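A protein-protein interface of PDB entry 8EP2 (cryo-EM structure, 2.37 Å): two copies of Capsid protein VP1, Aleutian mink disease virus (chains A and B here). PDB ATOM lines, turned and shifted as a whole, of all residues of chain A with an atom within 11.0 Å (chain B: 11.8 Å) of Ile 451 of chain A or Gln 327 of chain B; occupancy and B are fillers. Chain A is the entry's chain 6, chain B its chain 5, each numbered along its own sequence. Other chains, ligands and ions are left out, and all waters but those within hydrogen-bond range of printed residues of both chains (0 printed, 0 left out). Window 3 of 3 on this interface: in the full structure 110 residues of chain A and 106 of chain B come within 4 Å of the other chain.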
ATOM      1  N   ILE A 405       7.689 -31.180  14.684  1.00  0.00           N
ATOM      2  CA  ILE A 405       7.304 -29.963  15.380  1.00  0.00           C
ATOM      3  C   ILE A 405       8.471 -28.996  15.299  1.00  0.00           C
ATOM      4  O   ILE A 405       9.587 -29.337  15.697  1.00  0.00           O
ATOM      5  CB  ILE A 405       6.918 -30.248  16.838  1.00  0.00           C
ATOM      6  CG1 ILE A 405       5.689 -31.146  16.866  1.00  0.00           C
ATOM      7  CG2 ILE A 405       6.635 -28.968  17.562  1.00  0.00           C
ATOM      8  CD1 ILE A 405       5.371 -31.694  18.198  1.00  0.00           C
ATOM      9  N   TYR A 406       8.218 -27.797  14.785  1.00  0.00           N
ATOM     10  CA  TYR A 406       9.301 -26.931  14.351  1.00  0.00           C
ATOM     11  C   TYR A 406       8.919 -25.472  14.534  1.00  0.00           C
ATOM     12  O   TYR A 406       7.747 -25.127  14.678  1.00  0.00           O
ATOM     13  CB  TYR A 406       9.673 -27.248  12.900  1.00  0.00           C
ATOM     14  CG  TYR A 406       8.479 -27.319  11.993  1.00  0.00           C
ATOM     15  CD1 TYR A 406       8.027 -26.207  11.320  1.00  0.00           C
ATOM     16  CD2 TYR A 406       7.791 -28.509  11.832  1.00  0.00           C
ATOM     17  CE1 TYR A 406       6.935 -26.280  10.508  1.00  0.00           C
ATOM     18  CE2 TYR A 406       6.702 -28.587  11.030  1.00  0.00           C
ATOM     19  CZ  TYR A 406       6.275 -27.471  10.367  1.00  0.00           C
ATOM     20  OH  TYR A 406       5.178 -27.562   9.556  1.00  0.00           O
ATOM     21  N   ASP A 407       9.940 -24.619  14.536  1.00  0.00           N
ATOM     22  CA  ASP A 407       9.820 -23.194  14.784  1.00  0.00           C
ATOM     23  C   ASP A 407       9.943 -22.404  13.485  1.00  0.00           C
ATOM     24  O   ASP A 407      10.004 -22.962  12.391  1.00  0.00           O
ATOM     25  CB  ASP A 407      10.857 -22.744  15.811  1.00  0.00           C
ATOM     26  CG  ASP A 407      12.288 -22.931  15.335  1.00  0.00           C
ATOM     27  OD1 ASP A 407      12.521 -23.253  14.155  1.00  0.00           O
ATOM     28  OD2 ASP A 407      13.199 -22.744  16.157  1.00  0.00           O
ATOM     29  N   ARG A 408       9.993 -21.080  13.613  1.00  0.00           N
ATOM     30  CA  ARG A 408       9.949 -20.204  12.452  1.00  0.00           C
ATOM     31  C   ARG A 408      11.137 -20.412  11.529  1.00  0.00           C
ATOM     32  O   ARG A 408      10.985 -20.380  10.306  1.00  0.00           O
ATOM     33  CB  ARG A 408       9.902 -18.755  12.909  1.00  0.00           C
ATOM     34  CG  ARG A 408       9.642 -17.770  11.813  1.00  0.00           C
ATOM     35  CD  ARG A 408       9.635 -16.374  12.365  1.00  0.00           C
ATOM     36  NE  ARG A 408      10.981 -15.915  12.667  1.00  0.00           N
ATOM     37  CZ  ARG A 408      11.733 -15.251  11.801  1.00  0.00           C
ATOM     38  NH1 ARG A 408      12.953 -14.866  12.125  1.00  0.00           N
ATOM     39  NH2 ARG A 408      11.245 -14.939  10.616  1.00  0.00           N
ATOM     40  N   ASN A 414       5.326 -18.135  11.347  1.00  0.00           N
ATOM     41  CA  ASN A 414       5.461 -17.790  12.755  1.00  0.00           C
ATOM     42  C   ASN A 414       4.154 -17.928  13.524  1.00  0.00           C
ATOM     43  O   ASN A 414       4.141 -17.706  14.735  1.00  0.00           O
ATOM     44  CB  ASN A 414       6.016 -16.379  12.902  1.00  0.00           C
ATOM     45  CG  ASN A 414       6.591 -16.122  14.273  1.00  0.00           C
ATOM     46  OD1 ASN A 414       7.077 -17.034  14.933  1.00  0.00           O
ATOM     47  ND2 ASN A 414       6.553 -14.873  14.706  1.00  0.00           N
ATOM     48  N   GLU A 415       3.062 -18.269  12.854  1.00  0.00           N
ATOM     49  CA  GLU A 415       1.763 -18.442  13.478  1.00  0.00           C
ATOM     50  C   GLU A 415       1.348 -19.905  13.436  1.00  0.00           C
ATOM     51  O   GLU A 415       1.503 -20.574  12.410  1.00  0.00           O
ATOM     52  CB  GLU A 415       0.710 -17.593  12.770  1.00  0.00           C
ATOM     53  CG  GLU A 415      -0.657 -17.669  13.396  1.00  0.00           C
ATOM     54  CD  GLU A 415      -1.672 -16.816  12.672  1.00  0.00           C
ATOM     55  OE1 GLU A 415      -1.307 -16.205  11.646  1.00  0.00           O
ATOM     56  OE2 GLU A 415      -2.834 -16.753  13.126  1.00  0.00           O
ATOM     57  N   VAL A 416       0.815 -20.396  14.553  1.00  0.00           N
ATOM     58  CA  VAL A 416       0.273 -21.747  14.591  1.00  0.00           C
ATOM     59  C   VAL A 416      -0.992 -21.799  13.749  1.00  0.00           C
ATOM     60  O   VAL A 416      -1.758 -20.831  13.678  1.00  0.00           O
ATOM     61  CB  VAL A 416      -0.002 -22.184  16.040  1.00  0.00           C
ATOM     62  CG1 VAL A 416      -1.087 -21.331  16.662  1.00  0.00           C
ATOM     63  CG2 VAL A 416      -0.379 -23.646  16.096  1.00  0.00           C
ATOM     64  N   PRO A 450       0.474 -16.651  30.398  1.00  0.00           N
ATOM     65  CA  PRO A 450      -0.058 -17.279  29.184  1.00  0.00           C
ATOM     66  C   PRO A 450       0.333 -16.524  27.918  1.00  0.00           C
ATOM     67  O   PRO A 450       0.137 -15.313  27.829  1.00  0.00           O
ATOM     68  CB  PRO A 450      -1.571 -17.233  29.402  1.00  0.00           C
ATOM     69  CG  PRO A 450      -1.778 -16.057  30.290  1.00  0.00           C
ATOM     70  CD  PRO A 450      -0.590 -16.031  31.210  1.00  0.00           C
ATOM     71  N   ILE A 451       0.891 -17.248  26.946  1.00  0.00           N
ATOM     72  CA  ILE A 451       1.307 -16.614  25.705  1.00  0.00           C
ATOM     73  C   ILE A 451       0.093 -16.301  24.840  1.00  0.00           C
ATOM     74  O   ILE A 451      -0.979 -16.901  24.969  1.00  0.00           O
ATOM     75  CB  ILE A 451       2.308 -17.504  24.951  1.00  0.00           C
ATOM     76  CG1 ILE A 451       1.665 -18.856  24.636  1.00  0.00           C
ATOM     77  CG2 ILE A 451       3.580 -17.673  25.756  1.00  0.00           C
ATOM     78  CD1 ILE A 451       2.497 -19.735  23.747  1.00  0.00           C
ATOM     79  N   HIS A 452       0.270 -15.337  23.944  1.00  0.00           N
ATOM     80  CA  HIS A 452      -0.716 -15.080  22.904  1.00  0.00           C
ATOM     81  C   HIS A 452      -0.514 -16.094  21.787  1.00  0.00           C
ATOM     82  O   HIS A 452       0.580 -16.185  21.219  1.00  0.00           O
ATOM     83  CB  HIS A 452      -0.582 -13.655  22.378  1.00  0.00           C
ATOM     84  CG  HIS A 452      -1.606 -13.298  21.348  1.00  0.00           C
ATOM     85  ND1 HIS A 452      -1.474 -12.206  20.516  1.00  0.00           N
ATOM     86  CD2 HIS A 452      -2.778 -13.885  21.016  1.00  0.00           C
ATOM     87  CE1 HIS A 452      -2.522 -12.138  19.715  1.00  0.00           C
ATOM     88  NE2 HIS A 452      -3.328 -13.144  19.997  1.00  0.00           N
ATOM     89  N   HIS A 453      -1.561 -16.869  21.497  1.00  0.00           N
ATOM     90  CA  HIS A 453      -1.548 -17.948  20.509  1.00  0.00           C
ATOM     91  C   HIS A 453      -0.316 -18.830  20.675  1.00  0.00           C
ATOM     92  O   HIS A 453       0.097 -19.115  21.802  1.00  0.00           O
ATOM     93  CB  HIS A 453      -1.661 -17.408  19.071  1.00  0.00           C
ATOM     94  CG  HIS A 453      -0.571 -16.465  18.665  1.00  0.00           C
ATOM     95  ND1 HIS A 453      -0.561 -15.136  19.025  1.00  0.00           N
ATOM     96  CD2 HIS A 453       0.543 -16.660  17.919  1.00  0.00           C
ATOM     97  CE1 HIS A 453       0.514 -14.552  18.528  1.00  0.00           C
ATOM     98  NE2 HIS A 453       1.201 -15.455  17.852  1.00  0.00           N
ATOM     99  N   SER A 454       0.282 -19.262  19.572  1.00  0.00           N
ATOM    100  CA  SER A 454       1.499 -20.053  19.629  1.00  0.00           C
ATOM    101  C   SER A 454       2.264 -19.856  18.335  1.00  0.00           C
ATOM    102  O   SER A 454       1.676 -19.647  17.274  1.00  0.00           O
ATOM    103  CB  SER A 454       1.204 -21.536  19.852  1.00  0.00           C
ATOM    104  OG  SER A 454       2.405 -22.282  19.861  1.00  0.00           O
ATOM    105  N   LYS A 455       3.583 -19.906  18.437  1.00  0.00           N
ATOM    106  CA  LYS A 455       4.449 -19.633  17.306  1.00  0.00           C
ATOM    107  C   LYS A 455       4.985 -20.882  16.624  1.00  0.00           C
ATOM    108  O   LYS A 455       5.787 -20.760  15.697  1.00  0.00           O
ATOM    109  CB  LYS A 455       5.599 -18.739  17.753  1.00  0.00           C
ATOM    110  CG  LYS A 455       5.129 -17.370  18.169  1.00  0.00           C
ATOM    111  CD  LYS A 455       6.250 -16.542  18.730  1.00  0.00           C
ATOM    112  CE  LYS A 455       5.752 -15.173  19.132  1.00  0.00           C
ATOM    113  NZ  LYS A 455       6.830 -14.372  19.766  1.00  0.00           N
ATOM    114  N   ILE A 456       4.583 -22.067  17.049  1.00  0.00           N
ATOM    115  CA  ILE A 456       5.157 -23.297  16.520  1.00  0.00           C
ATOM    116  C   ILE A 456       4.176 -23.974  15.579  1.00  0.00           C
ATOM    117  O   ILE A 456       2.959 -23.924  15.768  1.00  0.00           O
ATOM    118  CB  ILE A 456       5.566 -24.246  17.658  1.00  0.00           C
ATOM    119  CG1 ILE A 456       4.346 -24.607  18.486  1.00  0.00           C
ATOM    120  CG2 ILE A 456       6.604 -23.595  18.527  1.00  0.00           C
ATOM    121  CD1 ILE A 456       4.611 -25.667  19.486  1.00  0.00           C
ATOM    122  N   ASP A 457       4.717 -24.619  14.553  1.00  0.00           N
ATOM    123  CA  ASP A 457       3.943 -25.380  13.587  1.00  0.00           C
ATOM    124  C   ASP A 457       4.340 -26.842  13.651  1.00  0.00           C
ATOM    125  O   ASP A 457       5.431 -27.189  14.099  1.00  0.00           O
ATOM    126  CB  ASP A 457       4.137 -24.863  12.158  1.00  0.00           C
ATOM    127  CG  ASP A 457       3.301 -23.643  11.859  1.00  0.00           C
ATOM    128  OD1 ASP A 457       2.301 -23.422  12.560  1.00  0.00           O
ATOM    129  OD2 ASP A 457       3.640 -22.895  10.926  1.00  0.00           O
ATOM    130  N   LEU B 303      17.556 -29.734  26.059  1.00  0.00           N
ATOM    131  CA  LEU B 303      18.282 -28.607  26.621  1.00  0.00           C
ATOM    132  C   LEU B 303      17.707 -28.256  27.985  1.00  0.00           C
ATOM    133  O   LEU B 303      16.491 -28.154  28.144  1.00  0.00           O
ATOM    134  CB  LEU B 303      18.187 -27.407  25.691  1.00  0.00           C
ATOM    135  CG  LEU B 303      19.062 -26.201  26.007  1.00  0.00           C
ATOM    136  CD1 LEU B 303      20.414 -26.663  26.468  1.00  0.00           C
ATOM    137  CD2 LEU B 303      19.218 -25.364  24.778  1.00  0.00           C
ATOM    138  N   LEU B 323      14.008 -28.671  32.609  1.00  0.00           N
ATOM    139  CA  LEU B 323      13.958 -28.547  31.164  1.00  0.00           C
ATOM    140  C   LEU B 323      13.456 -27.178  30.744  1.00  0.00           C
ATOM    141  O   LEU B 323      12.736 -26.498  31.476  1.00  0.00           O
ATOM    142  CB  LEU B 323      13.059 -29.616  30.559  1.00  0.00           C
ATOM    143  CG  LEU B 323      13.698 -30.972  30.294  1.00  0.00           C
ATOM    144  CD1 LEU B 323      13.970 -31.730  31.575  1.00  0.00           C
ATOM    145  CD2 LEU B 323      12.827 -31.764  29.362  1.00  0.00           C
ATOM    146  N   ILE B 324      13.839 -26.786  29.541  1.00  0.00           N
ATOM    147  CA  ILE B 324      13.385 -25.550  28.928  1.00  0.00           C
ATOM    148  C   ILE B 324      12.330 -25.926  27.904  1.00  0.00           C
ATOM    149  O   ILE B 324      12.644 -26.528  26.875  1.00  0.00           O
ATOM    150  CB  ILE B 324      14.540 -24.799  28.266  1.00  0.00           C
ATOM    151  CG1 ILE B 324      15.573 -24.399  29.313  1.00  0.00           C
ATOM    152  CG2 ILE B 324      14.009 -23.602  27.517  1.00  0.00           C
ATOM    153  CD1 ILE B 324      16.862 -23.931  28.725  1.00  0.00           C
ATOM    154  N   TYR B 325      11.080 -25.579  28.166  1.00  0.00           N
ATOM    155  CA  TYR B 325      10.025 -25.879  27.219  1.00  0.00           C
ATOM    156  C   TYR B 325       9.752 -24.661  26.347  1.00  0.00           C
ATOM    157  O   TYR B 325      10.369 -23.607  26.493  1.00  0.00           O
ATOM    158  CB  TYR B 325       8.767 -26.340  27.943  1.00  0.00           C
ATOM    159  CG  TYR B 325       8.953 -27.619  28.707  1.00  0.00           C
ATOM    160  CD1 TYR B 325       8.908 -28.842  28.063  1.00  0.00           C
ATOM    161  CD2 TYR B 325       9.142 -27.611  30.076  1.00  0.00           C
ATOM    162  CE1 TYR B 325       9.072 -30.016  28.757  1.00  0.00           C
ATOM    163  CE2 TYR B 325       9.302 -28.778  30.778  1.00  0.00           C
ATOM    164  CZ  TYR B 325       9.265 -29.978  30.114  1.00  0.00           C
ATOM    165  OH  TYR B 325       9.426 -31.152  30.809  1.00  0.00           O
ATOM    166  N   ILE B 326       8.812 -24.818  25.422  1.00  0.00           N
ATOM    167  CA  ILE B 326       8.470 -23.757  24.481  1.00  0.00           C
ATOM    168  C   ILE B 326       7.550 -22.758  25.160  1.00  0.00           C
ATOM    169  O   ILE B 326       6.502 -23.131  25.695  1.00  0.00           O
ATOM    170  CB  ILE B 326       7.816 -24.326  23.218  1.00  0.00           C
ATOM    171  CG1 ILE B 326       8.794 -25.220  22.459  1.00  0.00           C
ATOM    172  CG2 ILE B 326       7.319 -23.203  22.340  1.00  0.00           C
ATOM    173  CD1 ILE B 326      10.026 -24.495  21.994  1.00  0.00           C
ATOM    174  N   GLN B 327       7.945 -21.487  25.137  1.00  0.00           N
ATOM    175  CA  GLN B 327       7.125 -20.398  25.655  1.00  0.00           C
ATOM    176  C   GLN B 327       6.666 -20.695  27.075  1.00  0.00           C
ATOM    177  O   GLN B 327       5.570 -20.319  27.492  1.00  0.00           O
ATOM    178  CB  GLN B 327       5.932 -20.141  24.739  1.00  0.00           C
ATOM    179  CG  GLN B 327       6.324 -19.785  23.315  1.00  0.00           C
ATOM    180  CD  GLN B 327       7.236 -18.584  23.246  1.00  0.00           C
ATOM    181  OE1 GLN B 327       7.050 -17.604  23.968  1.00  0.00           O
ATOM    182  NE2 GLN B 327       8.243 -18.659  22.386  1.00  0.00           N
ATOM    183  N   GLY B 328       7.511 -21.403  27.819  1.00  0.00           N
ATOM    184  CA  GLY B 328       7.156 -21.859  29.142  1.00  0.00           C
ATOM    185  C   GLY B 328       6.014 -22.844  29.194  1.00  0.00           C
ATOM    186  O   GLY B 328       5.559 -23.178  30.292  1.00  0.00           O
ATOM    187  N   GLN B 329       5.535 -23.326  28.051  1.00  0.00           N
ATOM    188  CA  GLN B 329       4.371 -24.196  28.012  1.00  0.00           C
ATOM    189  C   GLN B 329       4.822 -25.623  28.283  1.00  0.00           C
ATOM    190  O   GLN B 329       5.612 -26.185  27.518  1.00  0.00           O
ATOM    191  CB  GLN B 329       3.666 -24.094  26.664  1.00  0.00           C
ATOM    192  CG  GLN B 329       2.390 -24.887  26.594  1.00  0.00           C
ATOM    193  CD  GLN B 329       1.364 -24.382  27.579  1.00  0.00           C
ATOM    194  OE1 GLN B 329       1.162 -24.974  28.638  1.00  0.00           O
ATOM    195  NE2 GLN B 329       0.726 -23.270  27.246  1.00  0.00           N
ATOM    196  N   ASP B 330       4.314 -26.203  29.365  1.00  0.00           N
ATOM    197  CA  ASP B 330       4.798 -27.494  29.825  1.00  0.00           C
ATOM    198  C   ASP B 330       4.605 -28.557  28.757  1.00  0.00           C
ATOM    199  O   ASP B 330       3.586 -28.583  28.062  1.00  0.00           O
ATOM    200  CB  ASP B 330       4.071 -27.904  31.100  1.00  0.00           C
ATOM    201  CG  ASP B 330       4.447 -27.039  32.278  1.00  0.00           C
ATOM    202  OD1 ASP B 330       5.483 -26.349  32.197  1.00  0.00           O
ATOM    203  OD2 ASP B 330       3.702 -27.039  33.279  1.00  0.00           O
ATOM    204  N   ASN B 331       5.607 -29.418  28.616  1.00  0.00           N
ATOM    205  CA  ASN B 331       5.616 -30.596  27.764  1.00  0.00           C
ATOM    206  C   ASN B 331       5.780 -30.253  26.285  1.00  0.00           C
ATOM    207  O   ASN B 331       5.784 -31.168  25.465  1.00  0.00           O
ATOM    208  CB  ASN B 331       4.359 -31.458  27.948  1.00  0.00           C
ATOM    209  CG  ASN B 331       4.264 -32.053  29.335  1.00  0.00           C
ATOM    210  OD1 ASN B 331       5.271 -32.243  30.015  1.00  0.00           O
ATOM    211  ND2 ASN B 331       3.044 -32.336  29.771  1.00  0.00           N
ATOM    212  N   THR B 332       5.884 -28.981  25.909  1.00  0.00           N
ATOM    213  CA  THR B 332       5.978 -28.603  24.504  1.00  0.00           C
ATOM    214  C   THR B 332       7.436 -28.537  24.067  1.00  0.00           C
ATOM    215  O   THR B 332       8.206 -27.722  24.577  1.00  0.00           O
ATOM    216  CB  THR B 332       5.291 -27.265  24.263  1.00  0.00           C
ATOM    217  OG1 THR B 332       3.925 -27.360  24.670  1.00  0.00           O
ATOM    218  CG2 THR B 332       5.331 -26.929  22.800  1.00  0.00           C
ATOM    219  N   ARG B 333       7.802 -29.383  23.111  1.00  0.00           N
ATOM    220  CA  ARG B 333       9.157 -29.484  22.602  1.00  0.00           C
ATOM    221  C   ARG B 333       9.113 -29.474  21.085  1.00  0.00           C
ATOM    222  O   ARG B 333       8.087 -29.784  20.482  1.00  0.00           O
ATOM    223  CB  ARG B 333       9.831 -30.765  23.089  1.00  0.00           C
ATOM    224  CG  ARG B 333      10.002 -30.834  24.579  1.00  0.00           C
ATOM    225  CD  ARG B 333      10.521 -32.179  25.008  1.00  0.00           C
ATOM    226  NE  ARG B 333      11.821 -32.463  24.424  1.00  0.00           N
ATOM    227  CZ  ARG B 333      12.470 -33.607  24.577  1.00  0.00           C
ATOM    228  NH1 ARG B 333      13.645 -33.783  24.007  1.00  0.00           N
ATOM    229  NH2 ARG B 333      11.943 -34.569  25.311  1.00  0.00           N
ATOM    230  N   LEU B 334      10.233 -29.141  20.458  1.00  0.00           N
ATOM    231  CA  LEU B 334      10.320 -29.174  19.003  1.00  0.00           C
ATOM    232  C   LEU B 334      11.028 -30.468  18.654  1.00  0.00           C
ATOM    233  O   LEU B 334      12.241 -30.582  18.804  1.00  0.00           O
ATOM    234  CB  LEU B 334      11.092 -27.975  18.476  1.00  0.00           C
ATOM    235  CG  LEU B 334      10.536 -26.593  18.768  1.00  0.00           C
ATOM    236  CD1 LEU B 334      11.508 -25.564  18.272  1.00  0.00           C
ATOM    237  CD2 LEU B 334       9.199 -26.419  18.114  1.00  0.00           C
ATOM    238  N   GLY B 343      -2.570 -31.992  20.856  1.00  0.00           N
ATOM    239  CA  GLY B 343      -2.300 -30.755  21.559  1.00  0.00           C
ATOM    240  C   GLY B 343      -0.825 -30.532  21.811  1.00  0.00           C
ATOM    241  O   GLY B 343      -0.444 -29.662  22.599  1.00  0.00           O
ATOM    242  N   LYS B 344       0.011 -31.325  21.141  1.00  0.00           N
ATOM    243  CA  LYS B 344       1.443 -31.047  21.016  1.00  0.00           C
ATOM    244  C   LYS B 344       2.175 -31.144  22.349  1.00  0.00           C
ATOM    245  O   LYS B 344       2.990 -30.286  22.680  1.00  0.00           O
ATOM    246  CB  LYS B 344       1.688 -29.671  20.393  1.00  0.00           C
ATOM    247  CG  LYS B 344       1.242 -29.514  18.960  1.00  0.00           C
ATOM    248  CD  LYS B 344       1.572 -28.119  18.462  1.00  0.00           C
ATOM    249  CE  LYS B 344       1.217 -27.949  17.002  1.00  0.00           C
ATOM    250  NZ  LYS B 344      -0.256 -27.859  16.814  1.00  0.00           N
ATOM    251  N   LYS B 345       1.898 -32.182  23.118  1.00  0.00           N
ATOM    252  CA  LYS B 345       2.690 -32.489  24.301  1.00  0.00           C
ATOM    253  C   LYS B 345       3.423 -33.801  24.065  1.00  0.00           C
ATOM    254  O   LYS B 345       2.806 -34.868  24.028  1.00  0.00           O
ATOM    255  CB  LYS B 345       1.822 -32.558  25.548  1.00  0.00           C
ATOM    256  CG  LYS B 345       1.308 -31.236  26.022  1.00  0.00           C
ATOM    257  CD  LYS B 345       0.445 -31.433  27.241  1.00  0.00           C
ATOM    258  CE  LYS B 345      -0.025 -30.111  27.798  1.00  0.00           C
ATOM    259  NZ  LYS B 345      -0.927 -30.306  28.963  1.00  0.00           N
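N of Ile 326 of chain B is in hydrogen-bond range of O of Thr 332 of chain B (3.1 Å). The backbone NH (N) of Tyr 406 of chain A lies within hydrogen-bond range of the backbone carbonyl oxygen (O) of Asp 457 of chain A (2.9 Å).
O of Arg 333 of chain B touches CG2 of Ile 405 of chain A (3.4 Å). Ile 405 of chain A touches Leu 334 of chain B. Leu 334 of chain B touches Tyr 406 of chain A. Asp 407 of chain A touches Leu 334 of chain B (CB to CD1, 3.8 Å). Gln 327 of chain B touches Ile 451 of chain A. Ile 456 of chain A touches Ile 326 of chain B. Thr 332 of chain B touches Ile 456 of chain A (CG2 to CD1, 3.6 Å). Ile 456 of chain A touches Leu 334 of chain B.
Of the printed residues of chain B, Ile 451 of chain A touches Gln 327 (3.6 Å). Of the printed residues of chain A, Gln 327 of chain B touches Ile 451 (3.6 Å). No residue of chain B comes within 4 Å of Pro 450 of chain A. No residue of chain B comes within 4 Å of His 452 of chain A. No residue of chain B comes within 4 Å of Ser 454 of chain A. Of chain A, only Ile 456 (3.9 Å) comes within 4 Å of Ile 326 of chain B. No residue of chain A comes within 4 Å of Gln 329 of chain B. Of the printed residues of chain B, Tyr 406 of chain A touches Leu 334 (3.7 Å). Of the printed residues of chain B, Asp 407 of chain A touches Leu 334. Of the printed residues of chain B, Ile 405 of chain A touches Arg 333 (3.4 Å) and Leu 334 (3.4 Å). Printed residues of chain B within 4 Å of Ile 456 of chain A: Ile 326, Thr 332 and Leu 334. The nearest residue of chain B that does not touch Ile 451 of chain A is Gln 329 of chain B (5.2 Å). The nearest printed residue of chain A that does not touch Arg 333 of chain B is Ile 456 of chain A (5.5 Å).
Of the 16 printed residues of chain B, 5 touch a printed residue of chain A. Printed residues of chain B that touch a printed residue of chain A: Ile 326, Gln 327, Thr 332, Arg 333 and Leu 334. Hydrophobic or aromatic side chains of chain B that line the printed part of chain A: Ile 326 and Leu 334. Among the printed residues, no Asp or Glu carboxylate lies within 4 Å of a Lys or Arg side-chain nitrogen of the other chain.
No position is printed for both chains. Of the 8 pairs that touch across the chains among the printed residues, none has its exchanged pair printed and touching as well.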
